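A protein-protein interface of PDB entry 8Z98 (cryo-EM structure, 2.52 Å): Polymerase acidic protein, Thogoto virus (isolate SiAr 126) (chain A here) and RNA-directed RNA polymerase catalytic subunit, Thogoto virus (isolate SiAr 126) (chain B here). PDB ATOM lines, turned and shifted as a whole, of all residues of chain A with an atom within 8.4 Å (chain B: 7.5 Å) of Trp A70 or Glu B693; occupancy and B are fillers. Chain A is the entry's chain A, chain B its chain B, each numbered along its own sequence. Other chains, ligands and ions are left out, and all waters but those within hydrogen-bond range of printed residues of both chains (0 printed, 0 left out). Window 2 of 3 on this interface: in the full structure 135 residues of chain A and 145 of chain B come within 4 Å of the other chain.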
ATOM      1  N   PHE A  60     -10.169 -39.108   5.770  1.00  0.00           N
ATOM      2  CA  PHE A  60     -11.479 -38.536   6.036  1.00  0.00           C
ATOM      3  C   PHE A  60     -12.059 -38.984   7.369  1.00  0.00           C
ATOM      4  O   PHE A  60     -13.045 -38.399   7.826  1.00  0.00           O
ATOM      5  CB  PHE A  60     -12.456 -38.906   4.913  1.00  0.00           C
ATOM      6  CG  PHE A  60     -12.216 -38.168   3.627  1.00  0.00           C
ATOM      7  CD1 PHE A  60     -11.279 -37.152   3.556  1.00  0.00           C
ATOM      8  CD2 PHE A  60     -12.931 -38.493   2.488  1.00  0.00           C
ATOM      9  CE1 PHE A  60     -11.060 -36.475   2.372  1.00  0.00           C
ATOM     10  CE2 PHE A  60     -12.717 -37.820   1.303  1.00  0.00           C
ATOM     11  CZ  PHE A  60     -11.780 -36.811   1.245  1.00  0.00           C
ATOM     12  N   GLN A  63     -12.575 -36.511  10.926  1.00  0.00           N
ATOM     13  CA  GLN A  63     -12.254 -35.155  10.516  1.00  0.00           C
ATOM     14  C   GLN A  63     -13.537 -34.343  10.435  1.00  0.00           C
ATOM     15  O   GLN A  63     -14.614 -34.884  10.165  1.00  0.00           O
ATOM     16  CB  GLN A  63     -11.533 -35.132   9.166  1.00  0.00           C
ATOM     17  CG  GLN A  63     -10.661 -33.908   8.953  1.00  0.00           C
ATOM     18  CD  GLN A  63      -9.693 -34.076   7.801  1.00  0.00           C
ATOM     19  OE1 GLN A  63     -10.099 -34.219   6.649  1.00  0.00           O
ATOM     20  NE2 GLN A  63      -8.401 -34.059   8.109  1.00  0.00           N
ATOM     21  N   ASP A  64     -13.418 -33.042  10.689  1.00  0.00           N
ATOM     22  CA  ASP A  64     -14.580 -32.168  10.630  1.00  0.00           C
ATOM     23  C   ASP A  64     -15.207 -32.212   9.243  1.00  0.00           C
ATOM     24  O   ASP A  64     -14.512 -32.169   8.225  1.00  0.00           O
ATOM     25  CB  ASP A  64     -14.188 -30.738  10.999  1.00  0.00           C
ATOM     26  CG  ASP A  64     -13.818 -30.598  12.463  1.00  0.00           C
ATOM     27  OD1 ASP A  64     -14.353 -31.369  13.287  1.00  0.00           O
ATOM     28  OD2 ASP A  64     -12.996 -29.720  12.793  1.00  0.00           O
ATOM     29  N   ARG A  65     -16.538 -32.311   9.214  1.00  0.00           N
ATOM     30  CA  ARG A  65     -17.244 -32.537   7.958  1.00  0.00           C
ATOM     31  C   ARG A  65     -17.054 -31.385   6.980  1.00  0.00           C
ATOM     32  O   ARG A  65     -17.095 -31.594   5.764  1.00  0.00           O
ATOM     33  CB  ARG A  65     -18.729 -32.779   8.239  1.00  0.00           C
ATOM     34  CG  ARG A  65     -19.621 -32.801   7.009  1.00  0.00           C
ATOM     35  CD  ARG A  65     -19.323 -33.992   6.111  1.00  0.00           C
ATOM     36  NE  ARG A  65     -19.665 -35.263   6.736  1.00  0.00           N
ATOM     37  CZ  ARG A  65     -18.924 -36.360   6.650  1.00  0.00           C
ATOM     38  NH1 ARG A  65     -17.797 -36.379   5.959  1.00  0.00           N
ATOM     39  NH2 ARG A  65     -19.327 -37.466   7.269  1.00  0.00           N
ATOM     40  N   SER A  66     -16.831 -30.169   7.481  1.00  0.00           N
ATOM     41  CA  SER A  66     -16.661 -29.023   6.592  1.00  0.00           C
ATOM     42  C   SER A  66     -15.404 -29.163   5.737  1.00  0.00           C
ATOM     43  O   SER A  66     -15.431 -28.926   4.522  1.00  0.00           O
ATOM     44  CB  SER A  66     -16.621 -27.735   7.412  1.00  0.00           C
ATOM     45  OG  SER A  66     -15.615 -27.799   8.407  1.00  0.00           O
ATOM     46  N   THR A  67     -14.288 -29.556   6.355  1.00  0.00           N
ATOM     47  CA  THR A  67     -13.056 -29.742   5.593  1.00  0.00           C
ATOM     48  C   THR A  67     -13.171 -30.921   4.637  1.00  0.00           C
ATOM     49  O   THR A  67     -12.638 -30.878   3.521  1.00  0.00           O
ATOM     50  CB  THR A  67     -11.873 -29.931   6.540  1.00  0.00           C
ATOM     51  OG1 THR A  67     -12.095 -31.084   7.359  1.00  0.00           O
ATOM     52  CG2 THR A  67     -11.713 -28.712   7.424  1.00  0.00           C
ATOM     53  N   ILE A  68     -13.860 -31.983   5.058  1.00  0.00           N
ATOM     54  CA  ILE A  68     -14.096 -33.115   4.167  1.00  0.00           C
ATOM     55  C   ILE A  68     -14.891 -32.668   2.950  1.00  0.00           C
ATOM     56  O   ILE A  68     -14.600 -33.069   1.817  1.00  0.00           O
ATOM     57  CB  ILE A  68     -14.807 -34.250   4.927  1.00  0.00           C
ATOM     58  CG1 ILE A  68     -13.909 -34.784   6.043  1.00  0.00           C
ATOM     59  CG2 ILE A  68     -15.203 -35.366   3.976  1.00  0.00           C
ATOM     60  CD1 ILE A  68     -14.607 -35.746   6.969  1.00  0.00           C
ATOM     61  N   GLU A  69     -15.908 -31.831   3.164  1.00  0.00           N
ATOM     62  CA  GLU A  69     -16.696 -31.318   2.049  1.00  0.00           C
ATOM     63  C   GLU A  69     -15.851 -30.445   1.133  1.00  0.00           C
ATOM     64  O   GLU A  69     -15.992 -30.509  -0.092  1.00  0.00           O
ATOM     65  CB  GLU A  69     -17.905 -30.543   2.572  1.00  0.00           C
ATOM     66  CG  GLU A  69     -18.961 -31.419   3.229  1.00  0.00           C
ATOM     67  CD  GLU A  69     -19.640 -32.354   2.249  1.00  0.00           C
ATOM     68  OE1 GLU A  69     -19.653 -32.043   1.040  1.00  0.00           O
ATOM     69  OE2 GLU A  69     -20.157 -33.404   2.687  1.00  0.00           O
ATOM     70  N   TRP A  70     -14.968 -29.623   1.706  1.00  0.00           N
ATOM     71  CA  TRP A  70     -14.039 -28.862   0.871  1.00  0.00           C
ATOM     72  C   TRP A  70     -13.210 -29.782  -0.014  1.00  0.00           C
ATOM     73  O   TRP A  70     -13.133 -29.589  -1.233  1.00  0.00           O
ATOM     74  CB  TRP A  70     -13.090 -28.022   1.716  1.00  0.00           C
ATOM     75  CG  TRP A  70     -12.426 -26.986   0.878  1.00  0.00           C
ATOM     76  CD1 TRP A  70     -12.830 -26.551  -0.350  1.00  0.00           C
ATOM     77  CD2 TRP A  70     -11.146 -26.389   1.107  1.00  0.00           C
ATOM     78  NE1 TRP A  70     -11.933 -25.645  -0.852  1.00  0.00           N
ATOM     79  CE2 TRP A  70     -10.882 -25.536   0.019  1.00  0.00           C
ATOM     80  CE3 TRP A  70     -10.213 -26.465   2.146  1.00  0.00           C
ATOM     81  CZ2 TRP A  70      -9.730 -24.764  -0.059  1.00  0.00           C
ATOM     82  CZ3 TRP A  70      -9.074 -25.696   2.067  1.00  0.00           C
ATOM     83  CH2 TRP A  70      -8.837 -24.862   0.971  1.00  0.00           C
ATOM     84  N   ILE A  71     -12.559 -30.775   0.595  1.00  0.00           N
ATOM     85  CA  ILE A  71     -11.656 -31.644  -0.156  1.00  0.00           C
ATOM     86  C   ILE A  71     -12.421 -32.413  -1.222  1.00  0.00           C
ATOM     87  O   ILE A  71     -11.920 -32.633  -2.331  1.00  0.00           O
ATOM     88  CB  ILE A  71     -10.898 -32.585   0.799  1.00  0.00           C
ATOM     89  CG1 ILE A  71     -10.205 -31.778   1.898  1.00  0.00           C
ATOM     90  CG2 ILE A  71      -9.891 -33.421   0.035  1.00  0.00           C
ATOM     91  CD1 ILE A  71      -9.187 -32.566   2.693  1.00  0.00           C
ATOM     92  N   CYS A  72     -13.649 -32.827  -0.910  1.00  0.00           N
ATOM     93  CA  CYS A  72     -14.477 -33.494  -1.906  1.00  0.00           C
ATOM     94  C   CYS A  72     -14.835 -32.550  -3.050  1.00  0.00           C
ATOM     95  O   CYS A  72     -14.859 -32.961  -4.215  1.00  0.00           O
ATOM     96  CB  CYS A  72     -15.736 -34.053  -1.247  1.00  0.00           C
ATOM     97  SG  CYS A  72     -15.436 -35.469  -0.169  1.00  0.00           S
ATOM     98  N   SER A  73     -15.123 -31.284  -2.735  1.00  0.00           N
ATOM     99  CA  SER A  73     -15.452 -30.315  -3.776  1.00  0.00           C
ATOM    100  C   SER A  73     -14.263 -30.055  -4.691  1.00  0.00           C
ATOM    101  O   SER A  73     -14.428 -29.926  -5.909  1.00  0.00           O
ATOM    102  CB  SER A  73     -15.935 -29.012  -3.143  1.00  0.00           C
ATOM    103  OG  SER A  73     -14.879 -28.357  -2.463  1.00  0.00           O
ATOM    104  N   LYS A  74     -13.058 -29.964  -4.123  1.00  0.00           N
ATOM    105  CA  LYS A  74     -11.874 -29.743  -4.947  1.00  0.00           C
ATOM    106  C   LYS A  74     -11.630 -30.903  -5.900  1.00  0.00           C
ATOM    107  O   LYS A  74     -11.021 -30.720  -6.960  1.00  0.00           O
ATOM    108  CB  LYS A  74     -10.646 -29.516  -4.065  1.00  0.00           C
ATOM    109  CG  LYS A  74     -10.686 -28.230  -3.260  1.00  0.00           C
ATOM    110  CD  LYS A  74      -9.369 -27.989  -2.539  1.00  0.00           C
ATOM    111  CE  LYS A  74      -9.204 -28.924  -1.353  1.00  0.00           C
ATOM    112  NZ  LYS A  74      -7.969 -28.620  -0.578  1.00  0.00           N
ATOM    113  N   LYS A  75     -12.093 -32.100  -5.545  1.00  0.00           N
ATOM    114  CA  LYS A  75     -11.944 -33.284  -6.378  1.00  0.00           C
ATOM    115  C   LYS A  75     -13.217 -33.631  -7.138  1.00  0.00           C
ATOM    116  O   LYS A  75     -13.286 -34.701  -7.753  1.00  0.00           O
ATOM    117  CB  LYS A  75     -11.501 -34.469  -5.520  1.00  0.00           C
ATOM    118  CG  LYS A  75     -10.251 -34.185  -4.709  1.00  0.00           C
ATOM    119  CD  LYS A  75     -10.001 -35.259  -3.671  1.00  0.00           C
ATOM    120  CE  LYS A  75      -8.549 -35.255  -3.230  1.00  0.00           C
ATOM    121  NZ  LYS A  75      -8.130 -33.934  -2.689  1.00  0.00           N
ATOM    122  N   LYS A  76     -14.221 -32.751  -7.109  1.00  0.00           N
ATOM    123  CA  LYS A  76     -15.480 -32.949  -7.834  1.00  0.00           C
ATOM    124  C   LYS A  76     -16.155 -34.262  -7.443  1.00  0.00           C
ATOM    125  O   LYS A  76     -16.690 -34.983  -8.288  1.00  0.00           O
ATOM    126  CB  LYS A  76     -15.264 -32.878  -9.348  1.00  0.00           C
ATOM    127  CG  LYS A  76     -15.343 -31.473  -9.926  1.00  0.00           C
ATOM    128  CD  LYS A  76     -14.070 -30.686  -9.664  1.00  0.00           C
ATOM    129  CE  LYS A  76     -12.908 -31.230 -10.479  1.00  0.00           C
ATOM    130  NZ  LYS A  76     -11.671 -30.423 -10.288  1.00  0.00           N
ATOM    131  N   VAL A  77     -16.129 -34.577  -6.149  1.00  0.00           N
ATOM    132  CA  VAL A  77     -16.796 -35.755  -5.613  1.00  0.00           C
ATOM    133  C   VAL A  77     -17.661 -35.325  -4.437  1.00  0.00           C
ATOM    134  O   VAL A  77     -17.482 -34.250  -3.862  1.00  0.00           O
ATOM    135  CB  VAL A  77     -15.803 -36.856  -5.182  1.00  0.00           C
ATOM    136  CG1 VAL A  77     -14.997 -37.344  -6.375  1.00  0.00           C
ATOM    137  CG2 VAL A  77     -14.885 -36.346  -4.089  1.00  0.00           C
ATOM    138  N   GLN A  78     -18.618 -36.181  -4.090  1.00  0.00           N
ATOM    139  CA  GLN A  78     -19.565 -35.877  -3.022  1.00  0.00           C
ATOM    140  C   GLN A  78     -19.979 -37.177  -2.354  1.00  0.00           C
ATOM    141  O   GLN A  78     -20.569 -38.046  -3.004  1.00  0.00           O
ATOM    142  CB  GLN A  78     -20.784 -35.133  -3.571  1.00  0.00           C
ATOM    143  CG  GLN A  78     -21.787 -34.713  -2.516  1.00  0.00           C
ATOM    144  CD  GLN A  78     -21.203 -33.744  -1.511  1.00  0.00           C
ATOM    145  OE1 GLN A  78     -21.014 -32.565  -1.807  1.00  0.00           O
ATOM    146  NE2 GLN A  78     -20.912 -34.237  -0.313  1.00  0.00           N
ATOM    147  N   LYS B 685     -10.489 -23.676  15.718  1.00  0.00           N
ATOM    148  CA  LYS B 685      -9.240 -23.577  14.970  1.00  0.00           C
ATOM    149  C   LYS B 685      -9.399 -24.134  13.562  1.00  0.00           C
ATOM    150  O   LYS B 685      -8.959 -23.521  12.581  1.00  0.00           O
ATOM    151  CB  LYS B 685      -8.127 -24.315  15.713  1.00  0.00           C
ATOM    152  CG  LYS B 685      -6.753 -24.150  15.091  1.00  0.00           C
ATOM    153  CD  LYS B 685      -5.712 -24.973  15.831  1.00  0.00           C
ATOM    154  CE  LYS B 685      -5.371 -24.355  17.176  1.00  0.00           C
ATOM    155  NZ  LYS B 685      -4.270 -25.089  17.860  1.00  0.00           N
ATOM    156  N   ARG B 686     -10.035 -25.302  13.444  1.00  0.00           N
ATOM    157  CA  ARG B 686     -10.203 -25.922  12.135  1.00  0.00           C
ATOM    158  C   ARG B 686     -11.086 -25.074  11.229  1.00  0.00           C
ATOM    159  O   ARG B 686     -10.771 -24.885  10.046  1.00  0.00           O
ATOM    160  CB  ARG B 686     -10.783 -27.325  12.297  1.00  0.00           C
ATOM    161  CG  ARG B 686     -11.025 -28.057  10.990  1.00  0.00           C
ATOM    162  CD  ARG B 686      -9.720 -28.520  10.363  1.00  0.00           C
ATOM    163  NE  ARG B 686      -9.208 -27.554   9.400  1.00  0.00           N
ATOM    164  CZ  ARG B 686      -8.039 -27.657   8.785  1.00  0.00           C
ATOM    165  NH1 ARG B 686      -7.228 -28.678   9.009  1.00  0.00           N
ATOM    166  NH2 ARG B 686      -7.673 -26.713   7.923  1.00  0.00           N
ATOM    167  N   ARG B 687     -12.189 -24.544  11.763  1.00  0.00           N
ATOM    168  CA  ARG B 687     -13.068 -23.720  10.941  1.00  0.00           C
ATOM    169  C   ARG B 687     -12.395 -22.409  10.555  1.00  0.00           C
ATOM    170  O   ARG B 687     -12.555 -21.933   9.425  1.00  0.00           O
ATOM    171  CB  ARG B 687     -14.383 -23.461  11.671  1.00  0.00           C
ATOM    172  CG  ARG B 687     -15.264 -22.420  11.013  1.00  0.00           C
ATOM    173  CD  ARG B 687     -15.716 -22.881   9.638  1.00  0.00           C
ATOM    174  NE  ARG B 687     -16.545 -24.078   9.694  1.00  0.00           N
ATOM    175  CZ  ARG B 687     -17.865 -24.070   9.812  1.00  0.00           C
ATOM    176  NH1 ARG B 687     -18.542 -22.940   9.915  1.00  0.00           N
ATOM    177  NH2 ARG B 687     -18.522 -25.226   9.825  1.00  0.00           N
ATOM    178  N   LEU B 688     -11.636 -21.810  11.476  1.00  0.00           N
ATOM    179  CA  LEU B 688     -10.915 -20.587  11.154  1.00  0.00           C
ATOM    180  C   LEU B 688      -9.904 -20.830  10.046  1.00  0.00           C
ATOM    181  O   LEU B 688      -9.789 -20.025   9.116  1.00  0.00           O
ATOM    182  CB  LEU B 688     -10.229 -20.038  12.403  1.00  0.00           C
ATOM    183  CG  LEU B 688      -9.502 -18.703  12.242  1.00  0.00           C
ATOM    184  CD1 LEU B 688     -10.471 -17.609  11.834  1.00  0.00           C
ATOM    185  CD2 LEU B 688      -8.792 -18.333  13.533  1.00  0.00           C
ATOM    186  N   GLU B 689      -9.174 -21.947  10.114  1.00  0.00           N
ATOM    187  CA  GLU B 689      -8.293 -22.305   9.010  1.00  0.00           C
ATOM    188  C   GLU B 689      -9.083 -22.415   7.711  1.00  0.00           C
ATOM    189  O   GLU B 689      -8.836 -21.665   6.759  1.00  0.00           O
ATOM    190  CB  GLU B 689      -7.571 -23.616   9.319  1.00  0.00           C
ATOM    191  CG  GLU B 689      -6.398 -23.467  10.272  1.00  0.00           C
ATOM    192  CD  GLU B 689      -5.997 -24.779  10.915  1.00  0.00           C
ATOM    193  OE1 GLU B 689      -6.001 -25.812  10.215  1.00  0.00           O
ATOM    194  OE2 GLU B 689      -5.669 -24.779  12.119  1.00  0.00           O
ATOM    195  N   LEU B 690     -10.131 -23.244   7.710  1.00  0.00           N
ATOM    196  CA  LEU B 690     -10.933 -23.440   6.506  1.00  0.00           C
ATOM    197  C   LEU B 690     -11.352 -22.107   5.897  1.00  0.00           C
ATOM    198  O   LEU B 690     -11.276 -21.919   4.678  1.00  0.00           O
ATOM    199  CB  LEU B 690     -12.164 -24.280   6.840  1.00  0.00           C
ATOM    200  CG  LEU B 690     -13.061 -24.662   5.667  1.00  0.00           C
ATOM    201  CD1 LEU B 690     -12.315 -25.585   4.726  1.00  0.00           C
ATOM    202  CD2 LEU B 690     -14.335 -25.306   6.164  1.00  0.00           C
ATOM    203  N   VAL B 691     -11.757 -21.155   6.740  1.00  0.00           N
ATOM    204  CA  VAL B 691     -12.090 -19.821   6.247  1.00  0.00           C
ATOM    205  C   VAL B 691     -10.865 -19.149   5.637  1.00  0.00           C
ATOM    206  O   VAL B 691     -10.948 -18.533   4.568  1.00  0.00           O
ATOM    207  CB  VAL B 691     -12.701 -18.963   7.373  1.00  0.00           C
ATOM    208  CG1 VAL B 691     -12.948 -17.544   6.886  1.00  0.00           C
ATOM    209  CG2 VAL B 691     -13.997 -19.577   7.862  1.00  0.00           C
ATOM    210  N   VAL B 692      -9.707 -19.257   6.299  1.00  0.00           N
ATOM    211  CA  VAL B 692      -8.524 -18.524   5.844  1.00  0.00           C
ATOM    212  C   VAL B 692      -8.076 -19.010   4.470  1.00  0.00           C
ATOM    213  O   VAL B 692      -7.875 -18.209   3.549  1.00  0.00           O
ATOM    214  CB  VAL B 692      -7.383 -18.626   6.870  1.00  0.00           C
ATOM    215  CG1 VAL B 692      -6.148 -17.948   6.317  1.00  0.00           C
ATOM    216  CG2 VAL B 692      -7.778 -17.973   8.178  1.00  0.00           C
ATOM    217  N   GLU B 693      -7.909 -20.321   4.306  1.00  0.00           N
ATOM    218  CA  GLU B 693      -7.563 -20.844   2.986  1.00  0.00           C
ATOM    219  C   GLU B 693      -8.775 -21.180   2.118  1.00  0.00           C
ATOM    220  O   GLU B 693      -8.636 -21.936   1.153  1.00  0.00           O
ATOM    221  CB  GLU B 693      -6.608 -22.052   3.058  1.00  0.00           C
ATOM    222  CG  GLU B 693      -7.150 -23.326   3.660  1.00  0.00           C
ATOM    223  CD  GLU B 693      -6.966 -23.360   5.157  1.00  0.00           C
ATOM    224  OE1 GLU B 693      -6.671 -22.295   5.733  1.00  0.00           O
ATOM    225  OE2 GLU B 693      -7.122 -24.443   5.757  1.00  0.00           O
ATOM    226  N   ARG B 694      -9.950 -20.622   2.414  1.00  0.00           N
ATOM    227  CA  ARG B 694     -10.996 -20.461   1.408  1.00  0.00           C
ATOM    228  C   ARG B 694     -11.318 -18.987   1.178  1.00  0.00           C
ATOM    229  O   ARG B 694     -12.451 -18.635   0.851  1.00  0.00           O
ATOM    230  CB  ARG B 694     -12.269 -21.223   1.774  1.00  0.00           C
ATOM    231  CG  ARG B 694     -12.134 -22.730   1.803  1.00  0.00           C
ATOM    232  CD  ARG B 694     -13.457 -23.364   2.193  1.00  0.00           C
ATOM    233  NE  ARG B 694     -14.476 -23.149   1.176  1.00  0.00           N
ATOM    234  CZ  ARG B 694     -15.524 -22.351   1.322  1.00  0.00           C
ATOM    235  NH1 ARG B 694     -15.727 -21.675   2.440  1.00  0.00           N
ATOM    236  NH2 ARG B 694     -16.385 -22.220   0.316  1.00  0.00           N
ATOM    237  N   SER B 695     -10.324 -18.117   1.340  1.00  0.00           N
ATOM    238  CA  SER B 695     -10.513 -16.679   1.206  1.00  0.00           C
ATOM    239  C   SER B 695     -10.032 -16.137  -0.134  1.00  0.00           C
ATOM    240  O   SER B 695      -9.939 -14.916  -0.292  1.00  0.00           O
ATOM    241  CB  SER B 695      -9.801 -15.948   2.343  1.00  0.00           C
ATOM    242  OG  SER B 695      -8.397 -16.111   2.252  1.00  0.00           O
ATOM    243  N   ASP B 696      -9.728 -17.018  -1.092  1.00  0.00           N
ATOM    244  CA  ASP B 696      -9.244 -16.665  -2.427  1.00  0.00           C
ATOM    245  C   ASP B 696      -8.216 -15.538  -2.404  1.00  0.00           C
ATOM    246  O   ASP B 696      -8.244 -14.644  -3.256  1.00  0.00           O
ATOM    247  CB  ASP B 696     -10.416 -16.309  -3.356  1.00  0.00           C
ATOM    248  CG  ASP B 696     -11.248 -15.141  -2.852  1.00  0.00           C
ATOM    249  OD1 ASP B 696     -10.906 -13.981  -3.163  1.00  0.00           O
ATOM    250  OD2 ASP B 696     -12.247 -15.386  -2.146  1.00  0.00           O
ATOM    251  N   LEU B 697      -7.299 -15.579  -1.442  1.00  0.00           N
ATOM    252  CA  LEU B 697      -6.221 -14.611  -1.344  1.00  0.00           C
ATOM    253  C   LEU B 697      -4.913 -15.238  -1.815  1.00  0.00           C
ATOM    254  O   LEU B 697      -4.868 -16.381  -2.277  1.00  0.00           O
ATOM    255  CB  LEU B 697      -6.092 -14.090   0.090  1.00  0.00           C
ATOM    256  CG  LEU B 697      -7.256 -13.263   0.639  1.00  0.00           C
ATOM    257  CD1 LEU B 697      -7.032 -12.945   2.107  1.00  0.00           C
ATOM    258  CD2 LEU B 697      -7.435 -11.987  -0.167  1.00  0.00           C
ATOM    259  N   LYS B 702      -1.938 -16.124   3.146  1.00  0.00           N
ATOM    260  CA  LYS B 702      -2.550 -17.225   3.880  1.00  0.00           C
ATOM    261  C   LYS B 702      -1.561 -17.850   4.857  1.00  0.00           C
ATOM    262  O   LYS B 702      -1.915 -18.156   6.003  1.00  0.00           O
ATOM    263  CB  LYS B 702      -3.071 -18.270   2.894  1.00  0.00           C
ATOM    264  CG  LYS B 702      -4.300 -17.842   2.114  1.00  0.00           C
ATOM    265  CD  LYS B 702      -4.863 -19.013   1.336  1.00  0.00           C
ATOM    266  CE  LYS B 702      -6.075 -18.600   0.532  1.00  0.00           C
ATOM    267  NZ  LYS B 702      -6.661 -19.754  -0.192  1.00  0.00           N
ATOM    268  N   ILE B 705      -1.106 -15.606   7.808  1.00  0.00           N
ATOM    269  CA  ILE B 705      -2.267 -15.625   8.695  1.00  0.00           C
ATOM    270  C   ILE B 705      -2.282 -16.888   9.552  1.00  0.00           C
ATOM    271  O   ILE B 705      -2.491 -16.822  10.770  1.00  0.00           O
ATOM    272  CB  ILE B 705      -3.569 -15.464   7.890  1.00  0.00           C
ATOM    273  CG1 ILE B 705      -3.596 -14.100   7.198  1.00  0.00           C
ATOM    274  CG2 ILE B 705      -4.773 -15.610   8.800  1.00  0.00           C
ATOM    275  CD1 ILE B 705      -4.704 -13.937   6.178  1.00  0.00           C
ATOM    276  N   LEU B 706      -2.070 -18.060   8.937  1.00  0.00           N
ATOM    277  CA  LEU B 706      -2.007 -19.284   9.738  1.00  0.00           C
ATOM    278  C   LEU B 706      -0.826 -19.281  10.698  1.00  0.00           C
ATOM    279  O   LEU B 706      -0.871 -19.970  11.724  1.00  0.00           O
ATOM    280  CB  LEU B 706      -1.950 -20.545   8.868  1.00  0.00           C
ATOM    281  CG  LEU B 706      -3.197 -21.132   8.192  1.00  0.00           C
ATOM    282  CD1 LEU B 706      -3.720 -20.305   7.031  1.00  0.00           C
ATOM    283  CD2 LEU B 706      -2.907 -22.562   7.735  1.00  0.00           C
ATOM    284  N   ILE B 709      -2.041 -18.234  14.166  1.00  0.00           N
ATOM    285  CA  ILE B 709      -3.109 -18.994  14.810  1.00  0.00           C
ATOM    286  C   ILE B 709      -2.453 -19.975  15.776  1.00  0.00           C
ATOM    287  O   ILE B 709      -1.950 -21.023  15.372  1.00  0.00           O
ATOM    288  CB  ILE B 709      -3.991 -19.711  13.788  1.00  0.00           C
ATOM    289  CG1 ILE B 709      -4.577 -18.711  12.790  1.00  0.00           C
ATOM    290  CG2 ILE B 709      -5.100 -20.483  14.489  1.00  0.00           C
ATOM    291  CD1 ILE B 709      -5.600 -19.314  11.853  1.00  0.00           C
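O of Asp A64 is in hydrogen-bond range of OG1 of Thr A67 (2.8 Å). The backbone carbonyl oxygen (O) of Glu B689 lies close to the side-chain carboxylate (OE1) of Glu B693, at 2.5 Å. The guanidinium group (NH2) of Arg B686 is in salt-bridge range of the side-chain carboxylate (OE2) of Glu B693. The guanidinium group (NH2) of Arg B686 lies within salt-bridge range of the side-chain carboxylate (OE1) of Glu B689. The backbone carbonyl oxygen of Trp A70 sits at hydrogen-bond distance from the side-chain hydroxyl of Ser A73 (2.5 Å). The backbone carbonyl oxygen (O) of Glu B693 is in hydrogen-bond range of the side-chain amino group (NZ) of Lys B702, at 3.2 Å.
Asp A64 touches Arg B686. Arg B687 touches Ser A66. Ser A66 touches Leu B690. Thr A67 touches Arg B686 (CG2 to NE, 3.4 Å). Trp A70 touches Leu B690. Trp A70 touches Glu B693 (CH2 to O, 2.9 Å). CG of Arg B694 touches CE2 of Trp A70, at 3.6 Å.
Of chain B, only Leu B690, Glu B693 and Arg B694 come within 4 Å of Trp A70. Glu B693 touches one residue of chain A. Of the printed residues of chain A, Arg B687 touches Ser A66 (3.97 Å). Printed residues of chain A within 4 Å of Arg B686: Asp A64 and Thr A67. Printed residues of chain A within 4 Å of Arg B694: Trp A70. The nearest residue of chain B that does not touch Trp A70 is Lys B702 (5.7 Å).
Hydrophobic or aromatic side chains of chain A within 4 Å of the printed part of chain B: Trp A70. Of the 17 printed residues of chain B, 5 touch a printed residue of chain A. Hydrophobic or aromatic side chains of chain B that line the printed part of chain A: Leu B690. Along chain B the printed residues that touch a printed residue of chain A span positions 686 to 694. Among the printed residues, 7 pairs touch across the chains.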
